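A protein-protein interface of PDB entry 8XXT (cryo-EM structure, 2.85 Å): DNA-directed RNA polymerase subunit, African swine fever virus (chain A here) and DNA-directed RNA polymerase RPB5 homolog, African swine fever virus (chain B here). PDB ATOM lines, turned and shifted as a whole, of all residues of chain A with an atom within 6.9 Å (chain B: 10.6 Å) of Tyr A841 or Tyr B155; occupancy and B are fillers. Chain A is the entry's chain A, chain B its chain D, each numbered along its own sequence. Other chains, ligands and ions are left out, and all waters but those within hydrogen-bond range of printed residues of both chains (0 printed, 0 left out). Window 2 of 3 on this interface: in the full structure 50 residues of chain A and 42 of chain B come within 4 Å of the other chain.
OH of Tyr A841 sits at hydrogen-bond distance from O of Arg B153, 2.8 Å away. The side-chain carboxylate (OE1) of Glu B154 lies within salt-bridge range of the guanidinium group (NH1) of Arg A843, 2.8 Å away. The side-chain hydroxyl of Tyr A990 sits at hydrogen-bond distance from the guanidinium group of Arg B153, at 3.4 Å. OE2 of Glu B154 lies within hydrogen-bond range of OH of Tyr A990.
The guanidinium group (NH2) of Arg A843 lies within salt-bridge range of the side-chain carboxylate (OD2) of Asp A839, at 2.5 Å. O of Leu B151 is in hydrogen-bond range of N of Leu B156 (3.1 Å). NH1 of Arg B153 is in salt-bridge range of OE2 of Glu B154, 2.7 Å away.
OE1 of Glu B154 touches CD2 of Tyr A841, at 3.4 Å. Tyr B155 touches Tyr A841. Arg A843 touches Leu B156 (NH1 to CD1, 3.4 Å). Phe B150 touches Gln A853. Glu B154 touches Gln A853.
No residue of chain B comes within 4 Å of Asp A839. Printed residues of chain B within 4 Å of Tyr A841: Arg B153, Glu B154 and Tyr B155. Of chain B, only Glu B154 and Leu B156 come within 4 Å of Arg A843. Phe A975 touches none of the printed residues of chain B. Of the printed residues of chain B, Tyr A990 touches Arg B153 and Glu B154. Of the printed residues of chain A, Phe B150 touches Gln A853. Of the printed residues of chain A, Arg B153 touches Tyr A841 and Tyr A990. Printed residues of chain A within 4 Å of Glu B154: Tyr A841, Arg A843, Gln A853 and Tyr A990. Of chain A, only Tyr A841 comes within 4 Å of Tyr B155. Printed residues of chain A within 4 Å of Leu B156: Arg A843. The nearest residue of chain B that does not touch Tyr A841 is Gly B152 (5.4 Å). The nearest printed residue of chain A that does not touch Phe B150 is Tyr A990 (4.3 Å).
Of the 15 printed residues of chain A, 4 touch a printed residue of chain B. Hydrophobic or aromatic side chains of chain A that line the printed part of chain B: Tyr A841 and Tyr A990. Printed residues of chain B that touch a printed residue of chain A: Phe B150, Arg B153, Glu B154, Tyr B155 and Leu B156. Among the printed residues, Asp or Glu carboxylates within 4 Å of a Lys or Arg side-chain nitrogen of the other chain: Arg A843 with Glu B154 (2.8 Å).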
ATOM      1  N   VAL A 838      -2.804 -10.980  26.743  1.00  0.00           N
ATOM      2  CA  VAL A 838      -3.995 -11.741  26.388  1.00  0.00           C
ATOM      3  C   VAL A 838      -4.479 -11.296  25.016  1.00  0.00           C
ATOM      4  O   VAL A 838      -4.719 -10.106  24.784  1.00  0.00           O
ATOM      5  CB  VAL A 838      -5.089 -11.564  27.446  1.00  0.00           C
ATOM      6  CG1 VAL A 838      -6.422 -12.016  26.905  1.00  0.00           C
ATOM      7  CG2 VAL A 838      -4.744 -12.341  28.690  1.00  0.00           C
ATOM      8  N   ASP A 839      -4.634 -12.248  24.103  1.00  0.00           N
ATOM      9  CA  ASP A 839      -5.085 -11.960  22.754  1.00  0.00           C
ATOM     10  C   ASP A 839      -6.580 -12.236  22.631  1.00  0.00           C
ATOM     11  O   ASP A 839      -7.247 -12.632  23.586  1.00  0.00           O
ATOM     12  CB  ASP A 839      -4.280 -12.767  21.734  1.00  0.00           C
ATOM     13  CG  ASP A 839      -4.352 -14.250  21.981  1.00  0.00           C
ATOM     14  OD1 ASP A 839      -4.754 -14.640  23.090  1.00  0.00           O
ATOM     15  OD2 ASP A 839      -3.998 -15.027  21.072  1.00  0.00           O
ATOM     16  N   TYR A 840      -7.110 -12.031  21.426  1.00  0.00           N
ATOM     17  CA  TYR A 840      -8.552 -12.070  21.219  1.00  0.00           C
ATOM     18  C   TYR A 840      -9.154 -13.452  21.417  1.00  0.00           C
ATOM     19  O   TYR A 840     -10.379 -13.565  21.505  1.00  0.00           O
ATOM     20  CB  TYR A 840      -8.889 -11.550  19.829  1.00  0.00           C
ATOM     21  CG  TYR A 840      -8.604 -10.083  19.664  1.00  0.00           C
ATOM     22  CD1 TYR A 840      -9.374  -9.133  20.306  1.00  0.00           C
ATOM     23  CD2 TYR A 840      -7.554  -9.646  18.878  1.00  0.00           C
ATOM     24  CE1 TYR A 840      -9.115  -7.796  20.161  1.00  0.00           C
ATOM     25  CE2 TYR A 840      -7.290  -8.316  18.722  1.00  0.00           C
ATOM     26  CZ  TYR A 840      -8.071  -7.395  19.368  1.00  0.00           C
ATOM     27  OH  TYR A 840      -7.804  -6.060  19.215  1.00  0.00           O
ATOM     28  N   TYR A 841      -8.340 -14.494  21.481  1.00  0.00           N
ATOM     29  CA  TYR A 841      -8.812 -15.810  21.879  1.00  0.00           C
ATOM     30  C   TYR A 841      -8.726 -16.016  23.382  1.00  0.00           C
ATOM     31  O   TYR A 841      -9.006 -17.118  23.860  1.00  0.00           O
ATOM     32  CB  TYR A 841      -8.009 -16.895  21.165  1.00  0.00           C
ATOM     33  CG  TYR A 841      -8.346 -17.049  19.705  1.00  0.00           C
ATOM     34  CD1 TYR A 841      -7.997 -16.074  18.784  1.00  0.00           C
ATOM     35  CD2 TYR A 841      -9.003 -18.177  19.245  1.00  0.00           C
ATOM     36  CE1 TYR A 841      -8.299 -16.216  17.452  1.00  0.00           C
ATOM     37  CE2 TYR A 841      -9.309 -18.328  17.918  1.00  0.00           C
ATOM     38  CZ  TYR A 841      -8.956 -17.347  17.024  1.00  0.00           C
ATOM     39  OH  TYR A 841      -9.263 -17.500  15.693  1.00  0.00           O
ATOM     40  N   ARG A 842      -8.336 -14.979  24.124  1.00  0.00           N
ATOM     41  CA  ARG A 842      -8.106 -15.019  25.566  1.00  0.00           C
ATOM     42  C   ARG A 842      -6.983 -15.973  25.943  1.00  0.00           C
ATOM     43  O   ARG A 842      -6.862 -16.366  27.105  1.00  0.00           O
ATOM     44  CB  ARG A 842      -9.384 -15.359  26.333  1.00  0.00           C
ATOM     45  CG  ARG A 842     -10.390 -14.241  26.293  1.00  0.00           C
ATOM     46  CD  ARG A 842     -11.450 -14.380  27.350  1.00  0.00           C
ATOM     47  NE  ARG A 842     -12.208 -13.144  27.469  1.00  0.00           N
ATOM     48  CZ  ARG A 842     -13.276 -12.852  26.740  1.00  0.00           C
ATOM     49  NH1 ARG A 842     -13.757 -13.702  25.850  1.00  0.00           N
ATOM     50  NH2 ARG A 842     -13.874 -11.677  26.908  1.00  0.00           N
ATOM     51  N   ARG A 843      -6.156 -16.347  24.974  1.00  0.00           N
ATOM     52  CA  ARG A 843      -4.918 -17.038  25.271  1.00  0.00           C
ATOM     53  C   ARG A 843      -3.876 -16.035  25.745  1.00  0.00           C
ATOM     54  O   ARG A 843      -4.090 -14.824  25.734  1.00  0.00           O
ATOM     55  CB  ARG A 843      -4.407 -17.775  24.040  1.00  0.00           C
ATOM     56  CG  ARG A 843      -5.487 -18.434  23.227  1.00  0.00           C
ATOM     57  CD  ARG A 843      -4.944 -18.872  21.890  1.00  0.00           C
ATOM     58  NE  ARG A 843      -4.521 -17.735  21.084  1.00  0.00           N
ATOM     59  CZ  ARG A 843      -4.518 -17.722  19.760  1.00  0.00           C
ATOM     60  NH1 ARG A 843      -4.888 -18.780  19.060  1.00  0.00           N
ATOM     61  NH2 ARG A 843      -4.133 -16.622  19.123  1.00  0.00           N
ATOM     62  N   VAL A 844      -2.730 -16.550  26.166  1.00  0.00           N
ATOM     63  CA  VAL A 844      -1.599 -15.721  26.552  1.00  0.00           C
ATOM     64  C   VAL A 844      -0.451 -16.056  25.617  1.00  0.00           C
ATOM     65  O   VAL A 844      -0.005 -17.208  25.565  1.00  0.00           O
ATOM     66  CB  VAL A 844      -1.205 -15.935  28.018  1.00  0.00           C
ATOM     67  CG1 VAL A 844       0.011 -15.114  28.353  1.00  0.00           C
ATOM     68  CG2 VAL A 844      -2.355 -15.554  28.922  1.00  0.00           C
ATOM     69  N   GLN A 853      -2.890 -21.727  26.679  1.00  0.00           N
ATOM     70  CA  GLN A 853      -4.057 -21.932  25.832  1.00  0.00           C
ATOM     71  C   GLN A 853      -5.220 -21.062  26.278  1.00  0.00           C
ATOM     72  O   GLN A 853      -6.065 -20.686  25.460  1.00  0.00           O
ATOM     73  CB  GLN A 853      -4.460 -23.402  25.842  1.00  0.00           C
ATOM     74  CG  GLN A 853      -5.416 -23.779  24.739  1.00  0.00           C
ATOM     75  CD  GLN A 853      -4.818 -23.573  23.372  1.00  0.00           C
ATOM     76  OE1 GLN A 853      -4.014 -24.379  22.908  1.00  0.00           O
ATOM     77  NE2 GLN A 853      -5.204 -22.486  22.714  1.00  0.00           N
ATOM     78  N   LEU A 854      -5.281 -20.744  27.566  1.00  0.00           N
ATOM     79  CA  LEU A 854      -6.265 -19.830  28.122  1.00  0.00           C
ATOM     80  C   LEU A 854      -5.642 -19.224  29.366  1.00  0.00           C
ATOM     81  O   LEU A 854      -4.829 -19.869  30.030  1.00  0.00           O
ATOM     82  CB  LEU A 854      -7.578 -20.548  28.440  1.00  0.00           C
ATOM     83  CG  LEU A 854      -8.819 -19.699  28.685  1.00  0.00           C
ATOM     84  CD1 LEU A 854      -9.145 -18.866  27.469  1.00  0.00           C
ATOM     85  CD2 LEU A 854      -9.973 -20.606  29.022  1.00  0.00           C
ATOM     86  N   TYR A 855      -6.026 -17.986  29.677  1.00  0.00           N
ATOM     87  CA  TYR A 855      -5.253 -17.167  30.605  1.00  0.00           C
ATOM     88  C   TYR A 855      -5.034 -17.838  31.954  1.00  0.00           C
ATOM     89  O   TYR A 855      -3.892 -18.120  32.327  1.00  0.00           O
ATOM     90  CB  TYR A 855      -5.920 -15.811  30.817  1.00  0.00           C
ATOM     91  CG  TYR A 855      -5.461 -15.110  32.075  1.00  0.00           C
ATOM     92  CD1 TYR A 855      -4.116 -14.869  32.310  1.00  0.00           C
ATOM     93  CD2 TYR A 855      -6.373 -14.687  33.026  1.00  0.00           C
ATOM     94  CE1 TYR A 855      -3.698 -14.241  33.457  1.00  0.00           C
ATOM     95  CE2 TYR A 855      -5.960 -14.052  34.171  1.00  0.00           C
ATOM     96  CZ  TYR A 855      -4.622 -13.830  34.380  1.00  0.00           C
ATOM     97  OH  TYR A 855      -4.206 -13.198  35.525  1.00  0.00           O
ATOM     98  N   PHE A 975     -17.316 -17.909  26.235  1.00  0.00           N
ATOM     99  CA  PHE A 975     -15.958 -17.598  25.823  1.00  0.00           C
ATOM    100  C   PHE A 975     -15.890 -17.137  24.376  1.00  0.00           C
ATOM    101  O   PHE A 975     -14.944 -16.437  24.003  1.00  0.00           O
ATOM    102  CB  PHE A 975     -15.058 -18.814  26.023  1.00  0.00           C
ATOM    103  CG  PHE A 975     -14.839 -19.172  27.460  1.00  0.00           C
ATOM    104  CD1 PHE A 975     -14.003 -18.415  28.253  1.00  0.00           C
ATOM    105  CD2 PHE A 975     -15.468 -20.267  28.018  1.00  0.00           C
ATOM    106  CE1 PHE A 975     -13.802 -18.741  29.573  1.00  0.00           C
ATOM    107  CE2 PHE A 975     -15.269 -20.596  29.338  1.00  0.00           C
ATOM    108  CZ  PHE A 975     -14.435 -19.833  30.115  1.00  0.00           C
ATOM    109  N   TYR A 990     -10.501 -27.275  24.648  1.00  0.00           N
ATOM    110  CA  TYR A 990     -10.015 -26.539  25.808  1.00  0.00           C
ATOM    111  C   TYR A 990     -11.056 -25.581  26.363  1.00  0.00           C
ATOM    112  O   TYR A 990     -11.000 -25.248  27.550  1.00  0.00           O
ATOM    113  CB  TYR A 990      -8.728 -25.788  25.462  1.00  0.00           C
ATOM    114  CG  TYR A 990      -8.908 -24.545  24.622  1.00  0.00           C
ATOM    115  CD1 TYR A 990      -9.023 -24.624  23.245  1.00  0.00           C
ATOM    116  CD2 TYR A 990      -8.931 -23.289  25.207  1.00  0.00           C
ATOM    117  CE1 TYR A 990      -9.173 -23.493  22.480  1.00  0.00           C
ATOM    118  CE2 TYR A 990      -9.082 -22.152  24.449  1.00  0.00           C
ATOM    119  CZ  TYR A 990      -9.203 -22.259  23.086  1.00  0.00           C
ATOM    120  OH  TYR A 990      -9.354 -21.124  22.326  1.00  0.00           O
ATOM    121  N   LEU A 991     -12.000 -25.127  25.539  1.00  0.00           N
ATOM    122  CA  LEU A 991     -13.081 -24.291  26.044  1.00  0.00           C
ATOM    123  C   LEU A 991     -14.137 -25.108  26.771  1.00  0.00           C
ATOM    124  O   LEU A 991     -14.807 -24.589  27.668  1.00  0.00           O
ATOM    125  CB  LEU A 991     -13.716 -23.503  24.903  1.00  0.00           C
ATOM    126  CG  LEU A 991     -12.868 -22.346  24.385  1.00  0.00           C
ATOM    127  CD1 LEU A 991     -13.634 -21.552  23.357  1.00  0.00           C
ATOM    128  CD2 LEU A 991     -12.437 -21.459  25.533  1.00  0.00           C
ATOM    129  N   TYR A1037      -9.293  -8.675  26.455  1.00  0.00           N
ATOM    130  CA  TYR A1037      -8.297  -8.730  25.399  1.00  0.00           C
ATOM    131  C   TYR A1037      -7.268  -7.626  25.593  1.00  0.00           C
ATOM    132  O   TYR A1037      -7.608  -6.486  25.921  1.00  0.00           O
ATOM    133  CB  TYR A1037      -8.965  -8.578  24.037  1.00  0.00           C
ATOM    134  CG  TYR A1037     -10.100  -9.536  23.794  1.00  0.00           C
ATOM    135  CD1 TYR A1037     -10.011 -10.854  24.191  1.00  0.00           C
ATOM    136  CD2 TYR A1037     -11.256  -9.121  23.156  1.00  0.00           C
ATOM    137  CE1 TYR A1037     -11.037 -11.734  23.960  1.00  0.00           C
ATOM    138  CE2 TYR A1037     -12.289  -9.995  22.922  1.00  0.00           C
ATOM    139  CZ  TYR A1037     -12.172 -11.301  23.325  1.00  0.00           C
ATOM    140  OH  TYR A1037     -13.192 -12.188  23.100  1.00  0.00           O
ATOM    141  N   TYR A1426      -5.180  -2.000  22.282  1.00  0.00           N
ATOM    142  CA  TYR A1426      -5.055  -3.314  21.668  1.00  0.00           C
ATOM    143  C   TYR A1426      -5.920  -3.427  20.423  1.00  0.00           C
ATOM    144  O   TYR A1426      -5.507  -4.028  19.426  1.00  0.00           O
ATOM    145  CB  TYR A1426      -5.427  -4.399  22.672  1.00  0.00           C
ATOM    146  CG  TYR A1426      -4.973  -5.777  22.268  1.00  0.00           C
ATOM    147  CD1 TYR A1426      -3.629  -6.098  22.228  1.00  0.00           C
ATOM    148  CD2 TYR A1426      -5.888  -6.757  21.930  1.00  0.00           C
ATOM    149  CE1 TYR A1426      -3.208  -7.356  21.862  1.00  0.00           C
ATOM    150  CE2 TYR A1426      -5.477  -8.017  21.563  1.00  0.00           C
ATOM    151  CZ  TYR A1426      -4.136  -8.310  21.529  1.00  0.00           C
ATOM    152  OH  TYR A1426      -3.717  -9.563  21.162  1.00  0.00           O
ATOM    153  N   ALA B 147      -5.385 -31.791  14.591  1.00  0.00           N
ATOM    154  CA  ALA B 147      -4.508 -30.699  14.992  1.00  0.00           C
ATOM    155  C   ALA B 147      -4.581 -29.547  13.998  1.00  0.00           C
ATOM    156  O   ALA B 147      -4.583 -28.376  14.391  1.00  0.00           O
ATOM    157  CB  ALA B 147      -3.075 -31.204  15.129  1.00  0.00           C
ATOM    158  N   GLN B 148      -4.649 -29.862  12.704  1.00  0.00           N
ATOM    159  CA  GLN B 148      -4.734 -28.818  11.690  1.00  0.00           C
ATOM    160  C   GLN B 148      -6.046 -28.054  11.783  1.00  0.00           C
ATOM    161  O   GLN B 148      -6.069 -26.835  11.600  1.00  0.00           O
ATOM    162  CB  GLN B 148      -4.562 -29.417  10.297  1.00  0.00           C
ATOM    163  CG  GLN B 148      -4.827 -28.432   9.170  1.00  0.00           C
ATOM    164  CD  GLN B 148      -3.913 -27.226   9.227  1.00  0.00           C
ATOM    165  OE1 GLN B 148      -2.715 -27.351   9.483  1.00  0.00           O
ATOM    166  NE2 GLN B 148      -4.477 -26.045   8.997  1.00  0.00           N
ATOM    167  N   GLU B 149      -7.154 -28.746  12.053  1.00  0.00           N
ATOM    168  CA  GLU B 149      -8.423 -28.039  12.196  1.00  0.00           C
ATOM    169  C   GLU B 149      -8.434 -27.185  13.459  1.00  0.00           C
ATOM    170  O   GLU B 149      -8.977 -26.071  13.457  1.00  0.00           O
ATOM    171  CB  GLU B 149      -9.593 -29.025  12.179  1.00  0.00           C
ATOM    172  CG  GLU B 149      -9.790 -29.828  13.447  1.00  0.00           C
ATOM    173  CD  GLU B 149     -11.230 -30.238  13.666  1.00  0.00           C
ATOM    174  OE1 GLU B 149     -12.041 -29.374  14.060  1.00  0.00           O
ATOM    175  OE2 GLU B 149     -11.548 -31.426  13.446  1.00  0.00           O
ATOM    176  N   PHE B 150      -7.813 -27.674  14.537  1.00  0.00           N
ATOM    177  CA  PHE B 150      -7.667 -26.852  15.732  1.00  0.00           C
ATOM    178  C   PHE B 150      -6.858 -25.598  15.435  1.00  0.00           C
ATOM    179  O   PHE B 150      -7.212 -24.501  15.879  1.00  0.00           O
ATOM    180  CB  PHE B 150      -7.010 -27.662  16.849  1.00  0.00           C
ATOM    181  CG  PHE B 150      -6.299 -26.823  17.869  1.00  0.00           C
ATOM    182  CD1 PHE B 150      -7.009 -26.132  18.831  1.00  0.00           C
ATOM    183  CD2 PHE B 150      -4.921 -26.727  17.867  1.00  0.00           C
ATOM    184  CE1 PHE B 150      -6.358 -25.361  19.768  1.00  0.00           C
ATOM    185  CE2 PHE B 150      -4.268 -25.955  18.803  1.00  0.00           C
ATOM    186  CZ  PHE B 150      -4.987 -25.272  19.753  1.00  0.00           C
ATOM    187  N   LEU B 151      -5.766 -25.744  14.683  1.00  0.00           N
ATOM    188  CA  LEU B 151      -4.954 -24.588  14.320  1.00  0.00           C
ATOM    189  C   LEU B 151      -5.728 -23.627  13.429  1.00  0.00           C
ATOM    190  O   LEU B 151      -5.635 -22.405  13.591  1.00  0.00           O
ATOM    191  CB  LEU B 151      -3.676 -25.046  13.622  1.00  0.00           C
ATOM    192  CG  LEU B 151      -2.655 -25.786  14.481  1.00  0.00           C
ATOM    193  CD1 LEU B 151      -1.496 -26.253  13.625  1.00  0.00           C
ATOM    194  CD2 LEU B 151      -2.171 -24.898  15.606  1.00  0.00           C
ATOM    195  N   GLY B 152      -6.495 -24.161  12.480  1.00  0.00           N
ATOM    196  CA  GLY B 152      -7.251 -23.308  11.581  1.00  0.00           C
ATOM    197  C   GLY B 152      -8.309 -22.498  12.300  1.00  0.00           C
ATOM    198  O   GLY B 152      -8.532 -21.329  11.980  1.00  0.00           O
ATOM    199  N   ARG B 153      -8.985 -23.109  13.275  1.00  0.00           N
ATOM    200  CA  ARG B 153      -9.914 -22.342  14.097  1.00  0.00           C
ATOM    201  C   ARG B 153      -9.181 -21.280  14.902  1.00  0.00           C
ATOM    202  O   ARG B 153      -9.677 -20.160  15.066  1.00  0.00           O
ATOM    203  CB  ARG B 153     -10.693 -23.269  15.025  1.00  0.00           C
ATOM    204  CG  ARG B 153     -11.857 -22.593  15.722  1.00  0.00           C
ATOM    205  CD  ARG B 153     -11.613 -22.456  17.209  1.00  0.00           C
ATOM    206  NE  ARG B 153     -12.652 -21.660  17.849  1.00  0.00           N
ATOM    207  CZ  ARG B 153     -12.465 -20.921  18.932  1.00  0.00           C
ATOM    208  NH1 ARG B 153     -11.292 -20.871  19.540  1.00  0.00           N
ATOM    209  NH2 ARG B 153     -13.479 -20.212  19.416  1.00  0.00           N
ATOM    210  N   GLU B 154      -7.996 -21.611  15.410  1.00  0.00           N
ATOM    211  CA  GLU B 154      -7.230 -20.705  16.252  1.00  0.00           C
ATOM    212  C   GLU B 154      -6.359 -19.739  15.465  1.00  0.00           C
ATOM    213  O   GLU B 154      -5.785 -18.828  16.068  1.00  0.00           O
ATOM    214  CB  GLU B 154      -6.350 -21.506  17.213  1.00  0.00           C
ATOM    215  CG  GLU B 154      -7.119 -22.300  18.253  1.00  0.00           C
ATOM    216  CD  GLU B 154      -7.544 -21.456  19.433  1.00  0.00           C
ATOM    217  OE1 GLU B 154      -6.719 -20.654  19.917  1.00  0.00           O
ATOM    218  OE2 GLU B 154      -8.700 -21.596  19.884  1.00  0.00           O
ATOM    219  N   TYR B 155      -6.242 -19.912  14.149  1.00  0.00           N
ATOM    220  CA  TYR B 155      -5.382 -19.082  13.306  1.00  0.00           C
ATOM    221  C   TYR B 155      -3.947 -19.081  13.827  1.00  0.00           C
ATOM    222  O   TYR B 155      -3.362 -18.042  14.134  1.00  0.00           O
ATOM    223  CB  TYR B 155      -5.927 -17.656  13.198  1.00  0.00           C
ATOM    224  CG  TYR B 155      -7.028 -17.493  12.182  1.00  0.00           C
ATOM    225  CD1 TYR B 155      -7.005 -18.196  10.989  1.00  0.00           C
ATOM    226  CD2 TYR B 155      -8.089 -16.634  12.413  1.00  0.00           C
ATOM    227  CE1 TYR B 155      -8.009 -18.050  10.056  1.00  0.00           C
ATOM    228  CE2 TYR B 155      -9.097 -16.481  11.487  1.00  0.00           C
ATOM    229  CZ  TYR B 155      -9.052 -17.192  10.311  1.00  0.00           C
ATOM    230  OH  TYR B 155     -10.055 -17.046   9.385  1.00  0.00           O
ATOM    231  N   LEU B 156      -3.381 -20.280  13.926  1.00  0.00           N
ATOM    232  CA  LEU B 156      -2.044 -20.469  14.460  1.00  0.00           C
ATOM    233  C   LEU B 156      -1.221 -21.336  13.525  1.00  0.00           C
ATOM    234  O   LEU B 156      -1.739 -22.250  12.878  1.00  0.00           O
ATOM    235  CB  LEU B 156      -2.072 -21.127  15.840  1.00  0.00           C
ATOM    236  CG  LEU B 156      -2.657 -20.336  17.003  1.00  0.00           C
ATOM    237  CD1 LEU B 156      -2.759 -21.232  18.214  1.00  0.00           C
ATOM    238  CD2 LEU B 156      -1.799 -19.125  17.302  1.00  0.00           C
ATOM    239  N   GLN B 157       0.065 -21.036  13.456  1.00  0.00           N
ATOM    240  CA  GLN B 157       1.016 -21.939  12.843  1.00  0.00           C
ATOM    241  C   GLN B 157       1.446 -22.987  13.861  1.00  0.00           C
ATOM    242  O   GLN B 157       1.351 -22.763  15.068  1.00  0.00           O
ATOM    243  CB  GLN B 157       2.230 -21.170  12.334  1.00  0.00           C
ATOM    244  CG  GLN B 157       2.036 -20.535  10.974  1.00  0.00           C
ATOM    245  CD  GLN B 157       1.141 -19.319  11.030  1.00  0.00           C
ATOM    246  OE1 GLN B 157       0.034 -19.321  10.492  1.00  0.00           O
ATOM    247  NE2 GLN B 157       1.613 -18.270  11.693  1.00  0.00           N
ATOM    248  N   PRO B 158       1.915 -24.147  13.401  1.00  0.00           N
ATOM    249  CA  PRO B 158       2.371 -25.168  14.354  1.00  0.00           C
ATOM    250  C   PRO B 158       3.488 -24.692  15.261  1.00  0.00           C
ATOM    251  O   PRO B 158       3.623 -25.200  16.380  1.00  0.00           O
ATOM    252  CB  PRO B 158       2.831 -26.309  13.439  1.00  0.00           C
ATOM    253  CG  PRO B 158       2.041 -26.132  12.201  1.00  0.00           C
ATOM    254  CD  PRO B 158       1.891 -24.654  12.020  1.00  0.00           C
ATOM    255  N   GLN B 159       4.291 -23.728  14.818  1.00  0.00           N
ATOM    256  CA  GLN B 159       5.406 -23.239  15.616  1.00  0.00           C
ATOM    257  C   GLN B 159       4.994 -22.186  16.636  1.00  0.00           C
ATOM    258  O   GLN B 159       5.838 -21.753  17.426  1.00  0.00           O
ATOM    259  CB  GLN B 159       6.488 -22.667  14.700  1.00  0.00           C
ATOM    260  CG  GLN B 159       6.866 -23.584  13.554  1.00  0.00           C
ATOM    261  CD  GLN B 159       6.060 -23.304  12.303  1.00  0.00           C
ATOM    262  OE1 GLN B 159       5.356 -22.298  12.220  1.00  0.00           O
ATOM    263  NE2 GLN B 159       6.152 -24.198  11.326  1.00  0.00           N
ATOM    264  N   ASP B 160       3.734 -21.754  16.630  1.00  0.00           N
ATOM    265  CA  ASP B 160       3.259 -20.805  17.627  1.00  0.00           C
ATOM    266  C   ASP B 160       2.851 -21.472  18.931  1.00  0.00           C
ATOM    267  O   ASP B 160       2.689 -20.772  19.936  1.00  0.00           O
ATOM    268  CB  ASP B 160       2.075 -20.005  17.078  1.00  0.00           C
ATOM    269  CG  ASP B 160       2.503 -18.894  16.142  1.00  0.00           C
ATOM    270  OD1 ASP B 160       3.674 -18.471  16.214  1.00  0.00           O
ATOM    271  OD2 ASP B 160       1.666 -18.437  15.339  1.00  0.00           O
ATOM    272  N   LEU B 161       2.686 -22.790  18.944  1.00  0.00           N
ATOM    273  CA  LEU B 161       2.241 -23.500  20.131  1.00  0.00           C
ATOM    274  C   LEU B 161       3.385 -23.649  21.129  1.00  0.00           C
ATOM    275  O   LEU B 161       4.553 -23.410  20.820  1.00  0.00           O
ATOM    276  CB  LEU B 161       1.696 -24.874  19.757  1.00  0.00           C
ATOM    277  CG  LEU B 161       0.559 -24.906  18.741  1.00  0.00           C
ATOM    278  CD1 LEU B 161       0.067 -26.322  18.558  1.00  0.00           C
ATOM    279  CD2 LEU B 161      -0.571 -24.006  19.189  1.00  0.00           C
